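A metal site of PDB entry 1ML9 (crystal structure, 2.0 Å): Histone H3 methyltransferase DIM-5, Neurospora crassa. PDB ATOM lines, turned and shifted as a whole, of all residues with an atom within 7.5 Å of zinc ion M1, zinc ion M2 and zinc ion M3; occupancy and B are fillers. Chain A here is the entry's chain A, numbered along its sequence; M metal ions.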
ATOM      1  N   VAL A  48     -17.616  20.982  12.103  1.00  0.00           N
ATOM      2  CA  VAL A  48     -16.259  20.479  12.167  1.00  0.00           C
ATOM      3  C   VAL A  48     -15.325  21.459  12.897  1.00  0.00           C
ATOM      4  O   VAL A  48     -15.393  22.679  12.695  1.00  0.00           O
ATOM      5  CB  VAL A  48     -15.714  20.147  10.711  1.00  0.00           C
ATOM      6  CG1 VAL A  48     -16.462  20.948   9.665  1.00  0.00           C
ATOM      7  CG2 VAL A  48     -14.221  20.411  10.605  1.00  0.00           C
ATOM      8  N   GLY A  49     -14.479  20.913  13.773  1.00  0.00           N
ATOM      9  CA  GLY A  49     -13.522  21.719  14.507  1.00  0.00           C
ATOM     10  C   GLY A  49     -12.114  21.329  14.076  1.00  0.00           C
ATOM     11  O   GLY A  49     -11.916  20.205  13.619  1.00  0.00           O
ATOM     12  N   CYS A  50     -11.145  22.235  14.195  1.00  0.00           N
ATOM     13  CA  CYS A  50      -9.774  21.921  13.796  1.00  0.00           C
ATOM     14  C   CYS A  50      -9.207  20.852  14.722  1.00  0.00           C
ATOM     15  O   CYS A  50      -9.694  20.668  15.833  1.00  0.00           O
ATOM     16  CB  CYS A  50      -8.900  23.171  13.831  1.00  0.00           C
ATOM     17  SG  CYS A  50      -8.602  23.877  15.489  1.00  0.00           S
ATOM     18  N   SER A  51      -8.174  20.152  14.249  1.00  0.00           N
ATOM     19  CA  SER A  51      -7.559  19.094  15.043  1.00  0.00           C
ATOM     20  C   SER A  51      -6.151  19.459  15.496  1.00  0.00           C
ATOM     21  O   SER A  51      -5.305  18.594  15.702  1.00  0.00           O
ATOM     22  CB  SER A  51      -7.498  17.794  14.224  1.00  0.00           C
ATOM     23  OG  SER A  51      -6.789  17.992  13.018  1.00  0.00           O
ATOM     24  N   CYS A  52      -5.914  20.755  15.670  1.00  0.00           N
ATOM     25  CA  CYS A  52      -4.607  21.245  16.098  1.00  0.00           C
ATOM     26  C   CYS A  52      -4.100  20.576  17.366  1.00  0.00           C
ATOM     27  O   CYS A  52      -4.847  20.388  18.333  1.00  0.00           O
ATOM     28  CB  CYS A  52      -4.659  22.750  16.275  1.00  0.00           C
ATOM     29  SG  CYS A  52      -4.705  23.636  14.687  1.00  0.00           S
ATOM     30  N   ALA A  53      -2.811  20.203  17.346  1.00  0.00           N
ATOM     31  CA  ALA A  53      -2.197  19.550  18.478  1.00  0.00           C
ATOM     32  C   ALA A  53      -2.242  20.392  19.739  1.00  0.00           C
ATOM     33  O   ALA A  53      -2.653  19.914  20.798  1.00  0.00           O
ATOM     34  N   SER A  54      -1.802  21.648  19.627  1.00  0.00           N
ATOM     35  CA  SER A  54      -1.805  22.558  20.765  1.00  0.00           C
ATOM     36  C   SER A  54      -2.373  23.917  20.357  1.00  0.00           C
ATOM     37  O   SER A  54      -2.305  24.295  19.185  1.00  0.00           O
ATOM     38  CB  SER A  54      -0.390  22.726  21.307  1.00  0.00           C
ATOM     39  N   ASP A  55      -2.925  24.628  21.335  1.00  0.00           N
ATOM     40  CA  ASP A  55      -3.506  25.942  21.114  1.00  0.00           C
ATOM     41  C   ASP A  55      -2.600  26.848  20.298  1.00  0.00           C
ATOM     42  O   ASP A  55      -3.043  27.851  19.743  1.00  0.00           O
ATOM     43  CB  ASP A  55      -3.807  26.614  22.461  1.00  0.00           C
ATOM     44  CG  ASP A  55      -4.886  25.899  23.217  1.00  0.00           C
ATOM     45  OD1 ASP A  55      -5.190  24.748  22.846  1.00  0.00           O
ATOM     46  OD2 ASP A  55      -5.457  26.489  24.165  1.00  0.00           O
ATOM     47  N   GLU A  56      -1.320  26.500  20.211  1.00  0.00           N
ATOM     48  CA  GLU A  56      -0.362  27.299  19.473  1.00  0.00           C
ATOM     49  C   GLU A  56      -0.449  27.111  17.953  1.00  0.00           C
ATOM     50  O   GLU A  56      -0.258  28.073  17.200  1.00  0.00           O
ATOM     51  CB  GLU A  56       1.044  27.001  19.962  1.00  0.00           C
ATOM     52  N   GLU A  57      -0.728  25.892  17.496  1.00  0.00           N
ATOM     53  CA  GLU A  57      -0.812  25.642  16.061  1.00  0.00           C
ATOM     54  C   GLU A  57      -1.937  26.381  15.349  1.00  0.00           C
ATOM     55  O   GLU A  57      -1.834  26.720  14.162  1.00  0.00           O
ATOM     56  N   CYS A  58      -3.019  26.641  16.083  1.00  0.00           N
ATOM     57  CA  CYS A  58      -4.183  27.315  15.548  1.00  0.00           C
ATOM     58  C   CYS A  58      -3.924  28.682  14.904  1.00  0.00           C
ATOM     59  O   CYS A  58      -4.770  29.172  14.153  1.00  0.00           O
ATOM     60  CB  CYS A  58      -5.239  27.484  16.645  1.00  0.00           C
ATOM     61  SG  CYS A  58      -6.040  25.928  17.160  1.00  0.00           S
ATOM     62  N   MET A  59      -2.778  29.294  15.181  1.00  0.00           N
ATOM     63  CA  MET A  59      -2.501  30.603  14.578  1.00  0.00           C
ATOM     64  C   MET A  59      -1.762  30.516  13.263  1.00  0.00           C
ATOM     65  O   MET A  59      -1.349  31.535  12.703  1.00  0.00           O
ATOM     66  CB  MET A  59      -1.725  31.507  15.542  1.00  0.00           C
ATOM     67  CG  MET A  59      -0.804  30.811  16.510  1.00  0.00           C
ATOM     68  SD  MET A  59      -0.078  31.979  17.685  1.00  0.00           S
ATOM     69  CE  MET A  59      -0.286  31.086  19.243  1.00  0.00           C
ATOM     70  N   TYR A  60      -1.607  29.299  12.745  1.00  0.00           N
ATOM     71  CA  TYR A  60      -0.910  29.088  11.477  1.00  0.00           C
ATOM     72  C   TYR A  60      -1.840  28.655  10.344  1.00  0.00           C
ATOM     73  O   TYR A  60      -2.950  28.155  10.567  1.00  0.00           O
ATOM     74  CB  TYR A  60       0.202  28.065  11.663  1.00  0.00           C
ATOM     75  CG  TYR A  60       1.305  28.535  12.578  1.00  0.00           C
ATOM     76  CD1 TYR A  60       1.419  28.027  13.876  1.00  0.00           C
ATOM     77  CD2 TYR A  60       2.234  29.482  12.150  1.00  0.00           C
ATOM     78  CE1 TYR A  60       2.439  28.462  14.721  1.00  0.00           C
ATOM     79  CE2 TYR A  60       3.255  29.925  12.989  1.00  0.00           C
ATOM     80  CZ  TYR A  60       3.349  29.403  14.283  1.00  0.00           C
ATOM     81  OH  TYR A  60       4.366  29.817  15.117  1.00  0.00           O
ATOM     82  N   THR A  62      -2.073  26.216   8.790  1.00  0.00           N
ATOM     83  CA  THR A  62      -2.432  24.805   8.834  1.00  0.00           C
ATOM     84  C   THR A  62      -3.664  24.511   9.670  1.00  0.00           C
ATOM     85  O   THR A  62      -4.209  23.399   9.631  1.00  0.00           O
ATOM     86  CB  THR A  62      -1.276  23.954   9.384  1.00  0.00           C
ATOM     87  OG1 THR A  62      -1.263  24.034  10.821  1.00  0.00           O
ATOM     88  CG2 THR A  62       0.056  24.438   8.843  1.00  0.00           C
ATOM     89  N   CYS A  63      -4.119  25.480  10.449  1.00  0.00           N
ATOM     90  CA  CYS A  63      -5.303  25.267  11.263  1.00  0.00           C
ATOM     91  C   CYS A  63      -6.496  25.136  10.307  1.00  0.00           C
ATOM     92  O   CYS A  63      -6.661  25.944   9.386  1.00  0.00           O
ATOM     93  CB  CYS A  63      -5.491  26.436  12.230  1.00  0.00           C
ATOM     94  SG  CYS A  63      -7.004  26.344  13.242  1.00  0.00           S
ATOM     95  N   GLN A  64      -7.313  24.107  10.520  1.00  0.00           N
ATOM     96  CA  GLN A  64      -8.492  23.875   9.681  1.00  0.00           C
ATOM     97  C   GLN A  64      -9.422  25.069   9.655  1.00  0.00           C
ATOM     98  O   GLN A  64      -9.990  25.415   8.619  1.00  0.00           O
ATOM     99  CB  GLN A  64      -9.268  22.659  10.198  1.00  0.00           C
ATOM    100  CG  GLN A  64      -8.909  21.370   9.502  1.00  0.00           C
ATOM    101  CD  GLN A  64      -7.979  20.509  10.334  1.00  0.00           C
ATOM    102  OE1 GLN A  64      -7.762  20.763  11.520  1.00  0.00           O
ATOM    103  NE2 GLN A  64      -7.411  19.470   9.706  1.00  0.00           N
ATOM    104  N   CYS A  65      -9.569  25.701  10.811  1.00  0.00           N
ATOM    105  CA  CYS A  65     -10.435  26.860  10.976  1.00  0.00           C
ATOM    106  C   CYS A  65     -10.106  28.020  10.064  1.00  0.00           C
ATOM    107  O   CYS A  65     -10.990  28.747   9.623  1.00  0.00           O
ATOM    108  CB  CYS A  65     -10.403  27.296  12.436  1.00  0.00           C
ATOM    109  SG  CYS A  65     -11.211  26.056  13.484  1.00  0.00           S
ATOM    110  N   LEU A  66      -8.817  28.179   9.770  1.00  0.00           N
ATOM    111  CA  LEU A  66      -8.384  29.272   8.911  1.00  0.00           C
ATOM    112  C   LEU A  66      -8.322  28.832   7.454  1.00  0.00           C
ATOM    113  O   LEU A  66      -7.826  29.570   6.595  1.00  0.00           O
ATOM    114  CB  LEU A  66      -7.024  29.773   9.391  1.00  0.00           C
ATOM    115  CG  LEU A  66      -6.954  30.446  10.770  1.00  0.00           C
ATOM    116  CD1 LEU A  66      -7.273  29.470  11.892  1.00  0.00           C
ATOM    117  CD2 LEU A  66      -5.550  30.995  10.951  1.00  0.00           C
ATOM    118  N   TYR A 110     -12.247  34.345  11.146  1.00  0.00           N
ATOM    119  CA  TYR A 110     -12.488  32.915  11.358  1.00  0.00           C
ATOM    120  C   TYR A 110     -11.828  32.462  12.659  1.00  0.00           C
ATOM    121  O   TYR A 110     -10.590  32.385  12.745  1.00  0.00           O
ATOM    122  CB  TYR A 110     -11.941  32.119  10.169  1.00  0.00           C
ATOM    123  CG  TYR A 110     -12.745  32.323   8.909  1.00  0.00           C
ATOM    124  CD1 TYR A 110     -12.398  33.304   7.993  1.00  0.00           C
ATOM    125  CD2 TYR A 110     -13.879  31.548   8.651  1.00  0.00           C
ATOM    126  CE1 TYR A 110     -13.147  33.522   6.840  1.00  0.00           C
ATOM    127  CE2 TYR A 110     -14.645  31.758   7.517  1.00  0.00           C
ATOM    128  CZ  TYR A 110     -14.271  32.741   6.607  1.00  0.00           C
ATOM    129  OH  TYR A 110     -15.015  32.947   5.472  1.00  0.00           O
ATOM    130  N   GLU A 111     -12.651  32.174  13.654  1.00  0.00           N
ATOM    131  CA  GLU A 111     -12.193  31.758  14.969  1.00  0.00           C
ATOM    132  C   GLU A 111     -12.426  30.287  15.261  1.00  0.00           C
ATOM    133  O   GLU A 111     -13.129  29.593  14.515  1.00  0.00           O
ATOM    134  CB  GLU A 111     -12.930  32.561  16.053  1.00  0.00           C
ATOM    135  CG  GLU A 111     -12.463  33.985  16.250  1.00  0.00           C
ATOM    136  CD  GLU A 111     -12.848  34.523  17.611  1.00  0.00           C
ATOM    137  OE1 GLU A 111     -12.306  35.581  17.994  1.00  0.00           O
ATOM    138  OE2 GLU A 111     -13.678  33.909  18.306  1.00  0.00           O
ATOM    139  N   CYS A 112     -11.827  29.815  16.349  1.00  0.00           N
ATOM    140  CA  CYS A 112     -12.030  28.447  16.762  1.00  0.00           C
ATOM    141  C   CYS A 112     -13.380  28.465  17.470  1.00  0.00           C
ATOM    142  O   CYS A 112     -13.946  29.546  17.690  1.00  0.00           O
ATOM    143  CB  CYS A 112     -10.903  27.980  17.686  1.00  0.00           C
ATOM    144  SG  CYS A 112      -9.452  27.429  16.714  1.00  0.00           S
ATOM    145  N   HIS A 113     -13.911  27.303  17.830  1.00  0.00           N
ATOM    146  CA  HIS A 113     -15.245  27.276  18.412  1.00  0.00           C
ATOM    147  C   HIS A 113     -15.547  25.938  19.040  1.00  0.00           C
ATOM    148  O   HIS A 113     -14.668  25.066  19.124  1.00  0.00           O
ATOM    149  CB  HIS A 113     -16.236  27.494  17.271  1.00  0.00           C
ATOM    150  CG  HIS A 113     -15.871  26.746  16.030  1.00  0.00           C
ATOM    151  ND1 HIS A 113     -14.940  27.220  15.124  1.00  0.00           N
ATOM    152  CD2 HIS A 113     -16.212  25.515  15.600  1.00  0.00           C
ATOM    153  CE1 HIS A 113     -14.733  26.313  14.189  1.00  0.00           C
ATOM    154  NE2 HIS A 113     -15.495  25.270  14.456  1.00  0.00           N
ATOM    155  N   GLY A 115     -15.995  22.488  19.435  1.00  0.00           N
ATOM    156  CA  GLY A 115     -15.627  21.428  18.528  1.00  0.00           C
ATOM    157  C   GLY A 115     -14.140  21.299  18.285  1.00  0.00           C
ATOM    158  O   GLY A 115     -13.638  20.190  18.104  1.00  0.00           O
ATOM    159  N   CYS A 116     -13.429  22.423  18.288  1.00  0.00           N
ATOM    160  CA  CYS A 116     -11.984  22.391  18.069  1.00  0.00           C
ATOM    161  C   CYS A 116     -11.226  21.629  19.151  1.00  0.00           C
ATOM    162  O   CYS A 116     -11.637  21.602  20.310  1.00  0.00           O
ATOM    163  CB  CYS A 116     -11.438  23.808  17.964  1.00  0.00           C
ATOM    164  SG  CYS A 116     -12.035  24.664  16.488  1.00  0.00           S
ATOM    165  N   ALA A 117     -10.103  21.039  18.748  1.00  0.00           N
ATOM    166  CA  ALA A 117      -9.252  20.256  19.644  1.00  0.00           C
ATOM    167  C   ALA A 117      -8.384  21.128  20.557  1.00  0.00           C
ATOM    168  O   ALA A 117      -7.596  20.614  21.356  1.00  0.00           O
ATOM    169  CB  ALA A 117      -8.364  19.319  18.828  1.00  0.00           C
ATOM    170  N   CYS A 118      -8.516  22.443  20.410  1.00  0.00           N
ATOM    171  CA  CYS A 118      -7.749  23.369  21.235  1.00  0.00           C
ATOM    172  C   CYS A 118      -8.574  23.663  22.484  1.00  0.00           C
ATOM    173  O   CYS A 118      -9.724  23.220  22.598  1.00  0.00           O
ATOM    174  CB  CYS A 118      -7.469  24.649  20.462  1.00  0.00           C
ATOM    175  SG  CYS A 118      -8.955  25.427  19.754  1.00  0.00           S
ATOM    176  N   SER A 119      -7.995  24.409  23.421  1.00  0.00           N
ATOM    177  CA  SER A 119      -8.701  24.736  24.643  1.00  0.00           C
ATOM    178  C   SER A 119      -9.310  26.119  24.627  1.00  0.00           C
ATOM    179  O   SER A 119      -9.011  26.924  23.741  1.00  0.00           O
ATOM    180  N   ASP A 121      -8.545  28.439  25.986  1.00  0.00           N
ATOM    181  CA  ASP A 121      -7.440  29.378  25.961  1.00  0.00           C
ATOM    182  C   ASP A 121      -6.838  29.621  24.590  1.00  0.00           C
ATOM    183  O   ASP A 121      -5.874  30.368  24.464  1.00  0.00           O
ATOM    184  CB  ASP A 121      -6.349  28.902  26.919  1.00  0.00           C
ATOM    185  N   CYS A 122      -7.400  28.991  23.558  1.00  0.00           N
ATOM    186  CA  CYS A 122      -6.876  29.159  22.213  1.00  0.00           C
ATOM    187  C   CYS A 122      -6.782  30.638  21.820  1.00  0.00           C
ATOM    188  O   CYS A 122      -7.756  31.375  21.933  1.00  0.00           O
ATOM    189  CB  CYS A 122      -7.741  28.417  21.191  1.00  0.00           C
ATOM    190  SG  CYS A 122      -7.203  28.721  19.479  1.00  0.00           S
ATOM    191  N   PRO A 123      -5.610  31.066  21.340  1.00  0.00           N
ATOM    192  CA  PRO A 123      -5.405  32.464  20.932  1.00  0.00           C
ATOM    193  C   PRO A 123      -6.385  32.936  19.863  1.00  0.00           C
ATOM    194  O   PRO A 123      -6.459  34.126  19.572  1.00  0.00           O
ATOM    195  CB  PRO A 123      -3.955  32.488  20.422  1.00  0.00           C
ATOM    196  CG  PRO A 123      -3.589  31.056  20.169  1.00  0.00           C
ATOM    197  CD  PRO A 123      -4.396  30.248  21.157  1.00  0.00           C
ATOM    198  N   ASN A 124      -7.114  31.993  19.283  1.00  0.00           N
ATOM    199  CA  ASN A 124      -8.071  32.329  18.234  1.00  0.00           C
ATOM    200  C   ASN A 124      -9.501  32.122  18.670  1.00  0.00           C
ATOM    201  O   ASN A 124     -10.339  31.669  17.900  1.00  0.00           O
ATOM    202  CB  ASN A 124      -7.790  31.503  16.983  1.00  0.00           C
ATOM    203  CG  ASN A 124      -8.400  32.115  15.747  1.00  0.00           C
ATOM    204  OD1 ASN A 124      -8.420  33.333  15.597  1.00  0.00           O
ATOM    205  ND2 ASN A 124      -8.913  31.274  14.856  1.00  0.00           N
ATOM    206  N   ARG A 125      -9.780  32.472  19.924  1.00  0.00           N
ATOM    207  CA  ARG A 125     -11.123  32.365  20.483  1.00  0.00           C
ATOM    208  C   ARG A 125     -11.445  33.648  21.240  1.00  0.00           C
ATOM    209  O   ARG A 125     -12.288  33.658  22.128  1.00  0.00           O
ATOM    210  CB  ARG A 125     -11.219  31.175  21.440  1.00  0.00           C
ATOM    211  CG  ARG A 125     -11.136  29.806  20.781  1.00  0.00           C
ATOM    212  CD  ARG A 125     -11.112  28.696  21.822  1.00  0.00           C
ATOM    213  NE  ARG A 125     -11.016  27.372  21.223  1.00  0.00           N
ATOM    214  CZ  ARG A 125     -11.971  26.438  21.286  1.00  0.00           C
ATOM    215  NH1 ARG A 125     -13.108  26.685  21.914  1.00  0.00           N
ATOM    216  NH2 ARG A 125     -11.779  25.255  20.716  1.00  0.00           N
HETATM  217 ZN    ZN M   1      -7.869  26.811  18.289  1.00  0.00          ZN
HETATM  218 ZN    ZN M   2     -10.238  25.553  15.492  1.00  0.00          ZN
HETATM  219 ZN    ZN M   3      -6.583  24.968  15.061  1.00  0.00          ZN
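SG of Cys 116 binds zinc ion M2. Zinc ion M2 is bound by the side-chain sulfur (SG) of Cys 65 (2.3 Å). Zinc ion M2 is bound by the side-chain sulfur (SG) of Cys 50. The side-chain sulfur (SG) of Cys 112 binds zinc ion M2. Zinc ion M2 has four donor atoms within binding distance.
Zinc ion M1 is bound by SG of Cys 118 (2.3 Å). Zinc ion M1 is bound by the side-chain sulfur (SG) of Cys 112 (2.3 Å). The side-chain sulfur (SG) of Cys 58 is bound to zinc ion M1, at 2.3 Å. Zinc ion M1 is bound by SG of Cys 122, at 2.3 Å.
Zinc ion M3 is bound by SG of Cys 63 (2.3 Å), SG of Cys 52 (2.3 Å), SG of Cys 50 (2.3 Å) and SG of Cys 58 (2.4 Å). Zinc ion M3 has four donor atoms within binding distance.
Along chain A the residues within 4 Å of zinc ion M1 span positions 58 to 122. The nearest printed residue that does not touch zinc ion M1 is Cys 50 (4.1 Å).
Four residues have an atom within 4 Å of zinc ion M3: Cys 50, Cys 52, Cys 58 and Cys 63. The nearest printed residue that does not touch zinc ion M3 is Cys 112 (4.1 Å).
Of the 32 residues printed, 4 come within 4 Å of zinc ion M2. The nearest printed residue that does not touch zinc ion M2 is Cys 63 (4.02 Å).
N of His 113 lies close to SG of Cys 116, at 3.5 Å. N of Cys 65 lies close to SG of Cys 63, 3.6 Å away. The backbone carbonyl oxygen of Cys 118 lies within hydrogen-bond range of the guanidinium group of Arg 125, 3.5 Å away. The backbone NH of Cys 112 is in hydrogen-bond range of the backbone carbonyl oxygen of Asn 124 (2.8 Å). N of Ala 117 sits at hydrogen-bond distance from O of Cys 50 (3.0 Å). N of Asn 124 lies close to SG of Cys 122, at 3.3 Å. OD2 of Asp 55 lies within hydrogen-bond range of N of Cys 122.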
